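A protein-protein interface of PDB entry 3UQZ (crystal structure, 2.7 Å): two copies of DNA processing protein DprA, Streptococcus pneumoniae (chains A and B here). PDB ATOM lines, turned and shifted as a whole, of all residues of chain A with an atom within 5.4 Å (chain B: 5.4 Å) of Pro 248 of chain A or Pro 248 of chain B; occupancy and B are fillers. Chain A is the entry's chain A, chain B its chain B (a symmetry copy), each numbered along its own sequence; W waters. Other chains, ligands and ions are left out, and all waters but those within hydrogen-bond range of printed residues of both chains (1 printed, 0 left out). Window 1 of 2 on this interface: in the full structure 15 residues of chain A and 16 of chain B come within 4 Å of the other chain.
O of Ile 247 of chain A sits close to SG of Cys 259 of chain A (3.7 Å). The backbone NH (N) of Gly 249 of chain A sits at hydrogen-bond distance from a ring nitrogen (NE2) of His 260 of chain A (3.1 Å). O of Ser 256 of chain A lies close to ND1 of His 260 of chain A (3.4 Å). SG of Cys 259 of chain B lies close to O of Ile 247 of chain B. N of Gly 249 of chain B lies within hydrogen-bond range of NE2 of His 260 of chain B. The backbone carbonyl oxygen (O) of Ser 256 of chain B lies close to a ring nitrogen (ND1) of His 260 of chain B, 3.4 Å away.
Pro 248 of chain A touches Pro 248 of chain B (CB to CB, 3.9 Å). CG of Pro 248 of chain A touches NE2 of His 260 of chain B, at 3.5 Å. Gly 249 of chain A touches Pro 248 of chain B (O to C, 3.5 Å). Gly 249 of chain B touches Gly 249 of chain A (O to CA, 3.5 Å). Ile 263 of chain A touches Leu 269 of chain B (CG2 to CD1, 3.8 Å). CD2 of Leu 269 of chain A touches CB of His 260 of chain B, at 3.8 Å. CG2 of Ile 263 of chain B touches CD1 of Leu 269 of chain A (3.7 Å). Leu 269 of chain B touches Leu 269 of chain A. Ile 251 of chain B touches Thr 271 of chain A (CD1 to O, 3.3 Å). His 260 of chain B touches Thr 271 of chain A (ND1 to CG2, 3.8 Å).
Of the printed residues of chain B, Pro 248 of chain A touches Pro 248 (3.9 Å), Gly 249 (3.6 Å), Ile 251 (3.7 Å) and His 260 (3.5 Å). Printed residues of chain A within 4 Å of His 260 of chain B: Pro 248 (3.5 Å), Leu 269 (3.8 Å) and Thr 271 (3.8 Å). Of the printed residues of chain B, Ile 263 of chain A touches Ile 263 (3.9 Å) and Leu 269 (3.8 Å). Of the printed residues of chain B, Ile 251 of chain A touches Ile 247, Pro 248, Val 270 and Thr 271. Ser 256 of chain B touches none of the printed residues of chain A. The nearest residue of chain B that does not touch Pro 248 of chain A is Ser 250 of chain B (4.7 Å). The nearest residue of chain A that does not touch Pro 248 of chain B is Ser 250 of chain A (4.6 Å).
Hydrophobic or aromatic side chains of chain B within 4 Å of the printed part of chain A: Ile 247, Pro 248, Ile 251, His 260, Ile 263 and Leu 269. Among the printed residues, 21 pairs touch across the chains.
Ile 247 of chain A touches Ile 251 of chain B, and with the chains exchanged Ile 251 of chain A touches Ile 247 of chain B. Pro 248 of chain B touches its own counterpart, Pro 248 of chain A. Pro 248 of chain A touches His 260 of chain B, and with the chains exchanged His 260 of chain A touches Pro 248 of chain B. His 260 of chain A touches Thr 271 of chain B, and with the chains exchanged Thr 271 of chain A touches His 260 of chain B. Positions printed for both chains: 246, 247, 248, 249, 250, 251, 256, 259, 260, 263, 269, 270 and 271.
Water W1 lies within hydrogen-bond range of O of Pro 248 of chain B and N of Ile 251 of chain A.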
ATOM      1  N   ALA A 246     -22.414  24.655   2.111  1.00  0.00           N
ATOM      2  CA  ALA A 246     -21.883  24.352   0.788  1.00  0.00           C
ATOM      3  C   ALA A 246     -22.341  25.313  -0.296  1.00  0.00           C
ATOM      4  O   ALA A 246     -23.531  25.623  -0.391  1.00  0.00           O
ATOM      5  CB  ALA A 246     -22.190  22.918   0.415  1.00  0.00           C
ATOM      6  N   ILE A 247     -21.380  25.808  -1.098  1.00  0.00           N
ATOM      7  CA  ILE A 247     -21.632  26.698  -2.230  1.00  0.00           C
ATOM      8  C   ILE A 247     -21.852  25.810  -3.469  1.00  0.00           C
ATOM      9  O   ILE A 247     -20.954  25.026  -3.808  1.00  0.00           O
ATOM     10  CB  ILE A 247     -20.482  27.733  -2.442  1.00  0.00           C
ATOM     11  CG1 ILE A 247     -20.295  28.642  -1.198  1.00  0.00           C
ATOM     12  CG2 ILE A 247     -20.726  28.574  -3.713  1.00  0.00           C
ATOM     13  CD1 ILE A 247     -18.925  29.334  -1.100  1.00  0.00           C
ATOM     14  N   PRO A 248     -23.030  25.893  -4.141  1.00  0.00           N
ATOM     15  CA  PRO A 248     -23.253  25.041  -5.324  1.00  0.00           C
ATOM     16  C   PRO A 248     -22.540  25.550  -6.574  1.00  0.00           C
ATOM     17  O   PRO A 248     -22.028  26.670  -6.600  1.00  0.00           O
ATOM     18  CB  PRO A 248     -24.777  25.064  -5.496  1.00  0.00           C
ATOM     19  CG  PRO A 248     -25.197  26.381  -4.934  1.00  0.00           C
ATOM     20  CD  PRO A 248     -24.203  26.753  -3.864  1.00  0.00           C
ATOM     21  N   GLY A 249     -22.511  24.702  -7.589  1.00  0.00           N
ATOM     22  CA  GLY A 249     -21.912  25.009  -8.879  1.00  0.00           C
ATOM     23  C   GLY A 249     -22.531  24.201  -9.999  1.00  0.00           C
ATOM     24  O   GLY A 249     -23.579  23.575  -9.810  1.00  0.00           O
ATOM     25  N   SER A 250     -21.864  24.198 -11.167  1.00  0.00           N
ATOM     26  CA  SER A 250     -22.262  23.453 -12.357  1.00  0.00           C
ATOM     27  C   SER A 250     -22.220  21.964 -12.061  1.00  0.00           C
ATOM     28  O   SER A 250     -21.360  21.526 -11.303  1.00  0.00           O
ATOM     29  CB  SER A 250     -21.312  23.771 -13.511  1.00  0.00           C
ATOM     30  OG  SER A 250     -21.413  22.840 -14.579  1.00  0.00           O
ATOM     31  N   ILE A 251     -23.125  21.185 -12.666  1.00  0.00           N
ATOM     32  CA  ILE A 251     -23.138  19.723 -12.489  1.00  0.00           C
ATOM     33  C   ILE A 251     -22.282  19.044 -13.567  1.00  0.00           C
ATOM     34  O   ILE A 251     -22.100  17.818 -13.545  1.00  0.00           O
ATOM     35  CB  ILE A 251     -24.577  19.142 -12.408  1.00  0.00           C
ATOM     36  CG1 ILE A 251     -25.402  19.417 -13.687  1.00  0.00           C
ATOM     37  CG2 ILE A 251     -25.285  19.610 -11.144  1.00  0.00           C
ATOM     38  CD1 ILE A 251     -26.069  18.193 -14.231  1.00  0.00           C
ATOM     39  N   SER A 256     -17.764  20.762  -8.298  1.00  0.00           N
ATOM     40  CA  SER A 256     -18.642  20.949  -7.135  1.00  0.00           C
ATOM     41  C   SER A 256     -19.418  19.699  -6.704  1.00  0.00           C
ATOM     42  O   SER A 256     -20.375  19.815  -5.937  1.00  0.00           O
ATOM     43  CB  SER A 256     -19.579  22.132  -7.356  1.00  0.00           C
ATOM     44  OG  SER A 256     -18.864  23.354  -7.410  1.00  0.00           O
ATOM     45  N   CYS A 259     -19.621  19.187  -2.861  1.00  0.00           N
ATOM     46  CA  CYS A 259     -20.529  20.190  -2.295  1.00  0.00           C
ATOM     47  C   CYS A 259     -21.955  19.704  -2.453  1.00  0.00           C
ATOM     48  O   CYS A 259     -22.739  19.787  -1.511  1.00  0.00           O
ATOM     49  CB  CYS A 259     -20.352  21.541  -2.985  1.00  0.00           C
ATOM     50  SG  CYS A 259     -18.706  22.271  -2.811  1.00  0.00           S
ATOM     51  N   HIS A 260     -22.287  19.211  -3.661  1.00  0.00           N
ATOM     52  CA  HIS A 260     -23.605  18.706  -4.029  1.00  0.00           C
ATOM     53  C   HIS A 260     -23.964  17.477  -3.220  1.00  0.00           C
ATOM     54  O   HIS A 260     -25.090  17.393  -2.730  1.00  0.00           O
ATOM     55  CB  HIS A 260     -23.686  18.453  -5.541  1.00  0.00           C
ATOM     56  CG  HIS A 260     -23.561  19.695  -6.373  1.00  0.00           C
ATOM     57  ND1 HIS A 260     -23.232  19.625  -7.710  1.00  0.00           N
ATOM     58  CD2 HIS A 260     -23.717  20.998  -6.028  1.00  0.00           C
ATOM     59  CE1 HIS A 260     -23.202  20.877  -8.139  1.00  0.00           C
ATOM     60  NE2 HIS A 260     -23.480  21.738  -7.160  1.00  0.00           N
ATOM     61  N   ILE A 263     -24.768  18.628   0.419  1.00  0.00           N
ATOM     62  CA  ILE A 263     -26.105  19.242   0.474  1.00  0.00           C
ATOM     63  C   ILE A 263     -27.174  18.139   0.515  1.00  0.00           C
ATOM     64  O   ILE A 263     -28.098  18.215   1.327  1.00  0.00           O
ATOM     65  CB  ILE A 263     -26.337  20.273  -0.665  1.00  0.00           C
ATOM     66  CG1 ILE A 263     -25.447  21.505  -0.468  1.00  0.00           C
ATOM     67  CG2 ILE A 263     -27.817  20.678  -0.767  1.00  0.00           C
ATOM     68  CD1 ILE A 263     -25.183  22.317  -1.734  1.00  0.00           C
ATOM     69  N   LEU A 269     -27.182  24.630   1.783  1.00  0.00           N
ATOM     70  CA  LEU A 269     -26.801  25.238   0.511  1.00  0.00           C
ATOM     71  C   LEU A 269     -26.746  26.737   0.767  1.00  0.00           C
ATOM     72  O   LEU A 269     -27.712  27.294   1.296  1.00  0.00           O
ATOM     73  CB  LEU A 269     -27.838  24.914  -0.598  1.00  0.00           C
ATOM     74  CG  LEU A 269     -27.487  25.365  -2.037  1.00  0.00           C
ATOM     75  CD1 LEU A 269     -28.130  24.463  -3.053  1.00  0.00           C
ATOM     76  CD2 LEU A 269     -27.907  26.796  -2.302  1.00  0.00           C
ATOM     77  N   VAL A 270     -25.629  27.388   0.405  1.00  0.00           N
ATOM     78  CA  VAL A 270     -25.467  28.835   0.616  1.00  0.00           C
ATOM     79  C   VAL A 270     -25.176  29.581  -0.688  1.00  0.00           C
ATOM     80  O   VAL A 270     -24.440  29.079  -1.534  1.00  0.00           O
ATOM     81  CB  VAL A 270     -24.496  29.217   1.785  1.00  0.00           C
ATOM     82  CG1 VAL A 270     -25.025  28.726   3.135  1.00  0.00           C
ATOM     83  CG2 VAL A 270     -23.067  28.724   1.542  1.00  0.00           C
ATOM     84  N   THR A 271     -25.774  30.771  -0.857  1.00  0.00           N
ATOM     85  CA  THR A 271     -25.624  31.618  -2.055  1.00  0.00           C
ATOM     86  C   THR A 271     -25.004  32.976  -1.714  1.00  0.00           C
ATOM     87  O   THR A 271     -24.547  33.688  -2.610  1.00  0.00           O
ATOM     88  CB  THR A 271     -26.979  31.792  -2.788  1.00  0.00           C
ATOM     89  OG1 THR A 271     -27.864  32.557  -1.976  1.00  0.00           O
ATOM     90  CG2 THR A 271     -27.636  30.461  -3.145  1.00  0.00           C
ATOM     91  N   ALA B 246     -34.271  19.827  -8.203  1.00  0.00           N
ATOM     92  CA  ALA B 246     -33.601  21.012  -8.723  1.00  0.00           C
ATOM     93  C   ALA B 246     -32.138  20.773  -9.104  1.00  0.00           C
ATOM     94  O   ALA B 246     -31.387  20.152  -8.347  1.00  0.00           O
ATOM     95  CB  ALA B 246     -33.724  22.158  -7.743  1.00  0.00           C
ATOM     96  N   ILE B 247     -31.758  21.245 -10.307  1.00  0.00           N
ATOM     97  CA  ILE B 247     -30.400  21.164 -10.829  1.00  0.00           C
ATOM     98  C   ILE B 247     -29.676  22.451 -10.397  1.00  0.00           C
ATOM     99  O   ILE B 247     -30.135  23.550 -10.747  1.00  0.00           O
ATOM    100  CB  ILE B 247     -30.360  20.944 -12.375  1.00  0.00           C
ATOM    101  CG1 ILE B 247     -31.060  19.614 -12.780  1.00  0.00           C
ATOM    102  CG2 ILE B 247     -28.904  20.978 -12.896  1.00  0.00           C
ATOM    103  CD1 ILE B 247     -31.516  19.532 -14.254  1.00  0.00           C
ATOM    104  N   PRO B 248     -28.564  22.343  -9.619  1.00  0.00           N
ATOM    105  CA  PRO B 248     -27.862  23.560  -9.183  1.00  0.00           C
ATOM    106  C   PRO B 248     -27.023  24.204 -10.281  1.00  0.00           C
ATOM    107  O   PRO B 248     -26.782  23.596 -11.330  1.00  0.00           O
ATOM    108  CB  PRO B 248     -27.003  23.075  -8.016  1.00  0.00           C
ATOM    109  CG  PRO B 248     -26.747  21.667  -8.297  1.00  0.00           C
ATOM    110  CD  PRO B 248     -27.909  21.131  -9.090  1.00  0.00           C
ATOM    111  N   GLY B 249     -26.592  25.434 -10.018  1.00  0.00           N
ATOM    112  CA  GLY B 249     -25.748  26.215 -10.909  1.00  0.00           C
ATOM    113  C   GLY B 249     -24.869  27.185 -10.152  1.00  0.00           C
ATOM    114  O   GLY B 249     -24.744  27.088  -8.927  1.00  0.00           O
ATOM    115  N   SER B 250     -24.263  28.134 -10.880  1.00  0.00           N
ATOM    116  CA  SER B 250     -23.387  29.149 -10.306  1.00  0.00           C
ATOM    117  C   SER B 250     -24.214  30.095  -9.453  1.00  0.00           C
ATOM    118  O   SER B 250     -25.379  30.330  -9.770  1.00  0.00           O
ATOM    119  CB  SER B 250     -22.664  29.919 -11.409  1.00  0.00           C
ATOM    120  OG  SER B 250     -22.073  31.124 -10.948  1.00  0.00           O
ATOM    121  N   ILE B 251     -23.621  30.623  -8.370  1.00  0.00           N
ATOM    122  CA  ILE B 251     -24.293  31.579  -7.494  1.00  0.00           C
ATOM    123  C   ILE B 251     -24.007  33.002  -7.971  1.00  0.00           C
ATOM    124  O   ILE B 251     -24.544  33.964  -7.417  1.00  0.00           O
ATOM    125  CB  ILE B 251     -23.952  31.361  -5.987  1.00  0.00           C
ATOM    126  CG1 ILE B 251     -22.453  31.525  -5.677  1.00  0.00           C
ATOM    127  CG2 ILE B 251     -24.462  30.024  -5.488  1.00  0.00           C
ATOM    128  CD1 ILE B 251     -22.163  32.430  -4.516  1.00  0.00           C
ATOM    129  N   SER B 256     -29.743  30.433 -11.740  1.00  0.00           N
ATOM    130  CA  SER B 256     -30.206  29.304 -10.909  1.00  0.00           C
ATOM    131  C   SER B 256     -30.673  29.665  -9.467  1.00  0.00           C
ATOM    132  O   SER B 256     -30.787  28.764  -8.626  1.00  0.00           O
ATOM    133  CB  SER B 256     -29.138  28.215 -10.875  1.00  0.00           C
ATOM    134  OG  SER B 256     -28.963  27.642 -12.159  1.00  0.00           O
ATOM    135  N   CYS B 259     -33.797  27.708  -8.288  1.00  0.00           N
ATOM    136  CA  CYS B 259     -33.431  26.309  -8.026  1.00  0.00           C
ATOM    137  C   CYS B 259     -32.826  26.210  -6.633  1.00  0.00           C
ATOM    138  O   CYS B 259     -33.163  25.300  -5.876  1.00  0.00           O
ATOM    139  CB  CYS B 259     -32.447  25.795  -9.075  1.00  0.00           C
ATOM    140  SG  CYS B 259     -33.090  25.773 -10.767  1.00  0.00           S
ATOM    141  N   HIS B 260     -31.927  27.163  -6.305  1.00  0.00           N
ATOM    142  CA  HIS B 260     -31.228  27.231  -5.028  1.00  0.00           C
ATOM    143  C   HIS B 260     -32.190  27.515  -3.891  1.00  0.00           C
ATOM    144  O   HIS B 260     -32.091  26.868  -2.848  1.00  0.00           O
ATOM    145  CB  HIS B 260     -30.085  28.253  -5.087  1.00  0.00           C
ATOM    146  CG  HIS B 260     -28.999  27.900  -6.059  1.00  0.00           C
ATOM    147  ND1 HIS B 260     -28.123  28.859  -6.527  1.00  0.00           N
ATOM    148  CD2 HIS B 260     -28.689  26.707  -6.628  1.00  0.00           C
ATOM    149  CE1 HIS B 260     -27.310  28.224  -7.354  1.00  0.00           C
ATOM    150  NE2 HIS B 260     -27.615  26.927  -7.446  1.00  0.00           N
ATOM    151  N   ILE B 263     -34.220  24.260  -3.229  1.00  0.00           N
ATOM    152  CA  ILE B 263     -33.399  23.288  -2.484  1.00  0.00           C
ATOM    153  C   ILE B 263     -33.383  23.655  -0.989  1.00  0.00           C
ATOM    154  O   ILE B 263     -33.568  22.780  -0.143  1.00  0.00           O
ATOM    155  CB  ILE B 263     -31.975  23.126  -3.087  1.00  0.00           C
ATOM    156  CG1 ILE B 263     -32.043  22.458  -4.474  1.00  0.00           C
ATOM    157  CG2 ILE B 263     -31.049  22.319  -2.141  1.00  0.00           C
ATOM    158  CD1 ILE B 263     -30.859  22.710  -5.389  1.00  0.00           C
ATOM    159  N   LEU B 269     -31.774  18.255  -4.436  1.00  0.00           N
ATOM    160  CA  LEU B 269     -30.711  18.712  -5.334  1.00  0.00           C
ATOM    161  C   LEU B 269     -30.346  17.491  -6.176  1.00  0.00           C
ATOM    162  O   LEU B 269     -30.100  16.410  -5.621  1.00  0.00           O
ATOM    163  CB  LEU B 269     -29.480  19.196  -4.534  1.00  0.00           C
ATOM    164  CG  LEU B 269     -28.323  19.834  -5.336  1.00  0.00           C
ATOM    165  CD1 LEU B 269     -27.585  20.850  -4.515  1.00  0.00           C
ATOM    166  CD2 LEU B 269     -27.350  18.797  -5.849  1.00  0.00           C
ATOM    167  N   VAL B 270     -30.339  17.643  -7.500  1.00  0.00           N
ATOM    168  CA  VAL B 270     -30.010  16.530  -8.404  1.00  0.00           C
ATOM    169  C   VAL B 270     -28.810  16.853  -9.307  1.00  0.00           C
ATOM    170  O   VAL B 270     -28.673  17.986  -9.782  1.00  0.00           O
ATOM    171  CB  VAL B 270     -31.233  15.931  -9.176  1.00  0.00           C
ATOM    172  CG1 VAL B 270     -32.249  15.318  -8.219  1.00  0.00           C
ATOM    173  CG2 VAL B 270     -31.903  16.956 -10.094  1.00  0.00           C
ATOM    174  N   THR B 271     -27.929  15.856  -9.504  1.00  0.00           N
ATOM    175  CA  THR B 271     -26.724  15.976 -10.337  1.00  0.00           C
ATOM    176  C   THR B 271     -26.758  15.000 -11.522  1.00  0.00           C
ATOM    177  O   THR B 271     -26.013  15.189 -12.485  1.00  0.00           O
ATOM    178  CB  THR B 271     -25.448  15.786  -9.497  1.00  0.00           C
ATOM    179  OG1 THR B 271     -25.390  14.439  -9.018  1.00  0.00           O
ATOM    180  CG2 THR B 271     -25.356  16.770  -8.346  1.00  0.00           C
HETATM  181  O   HOH W   1     -25.249  23.579 -13.716  1.00  0.00           O
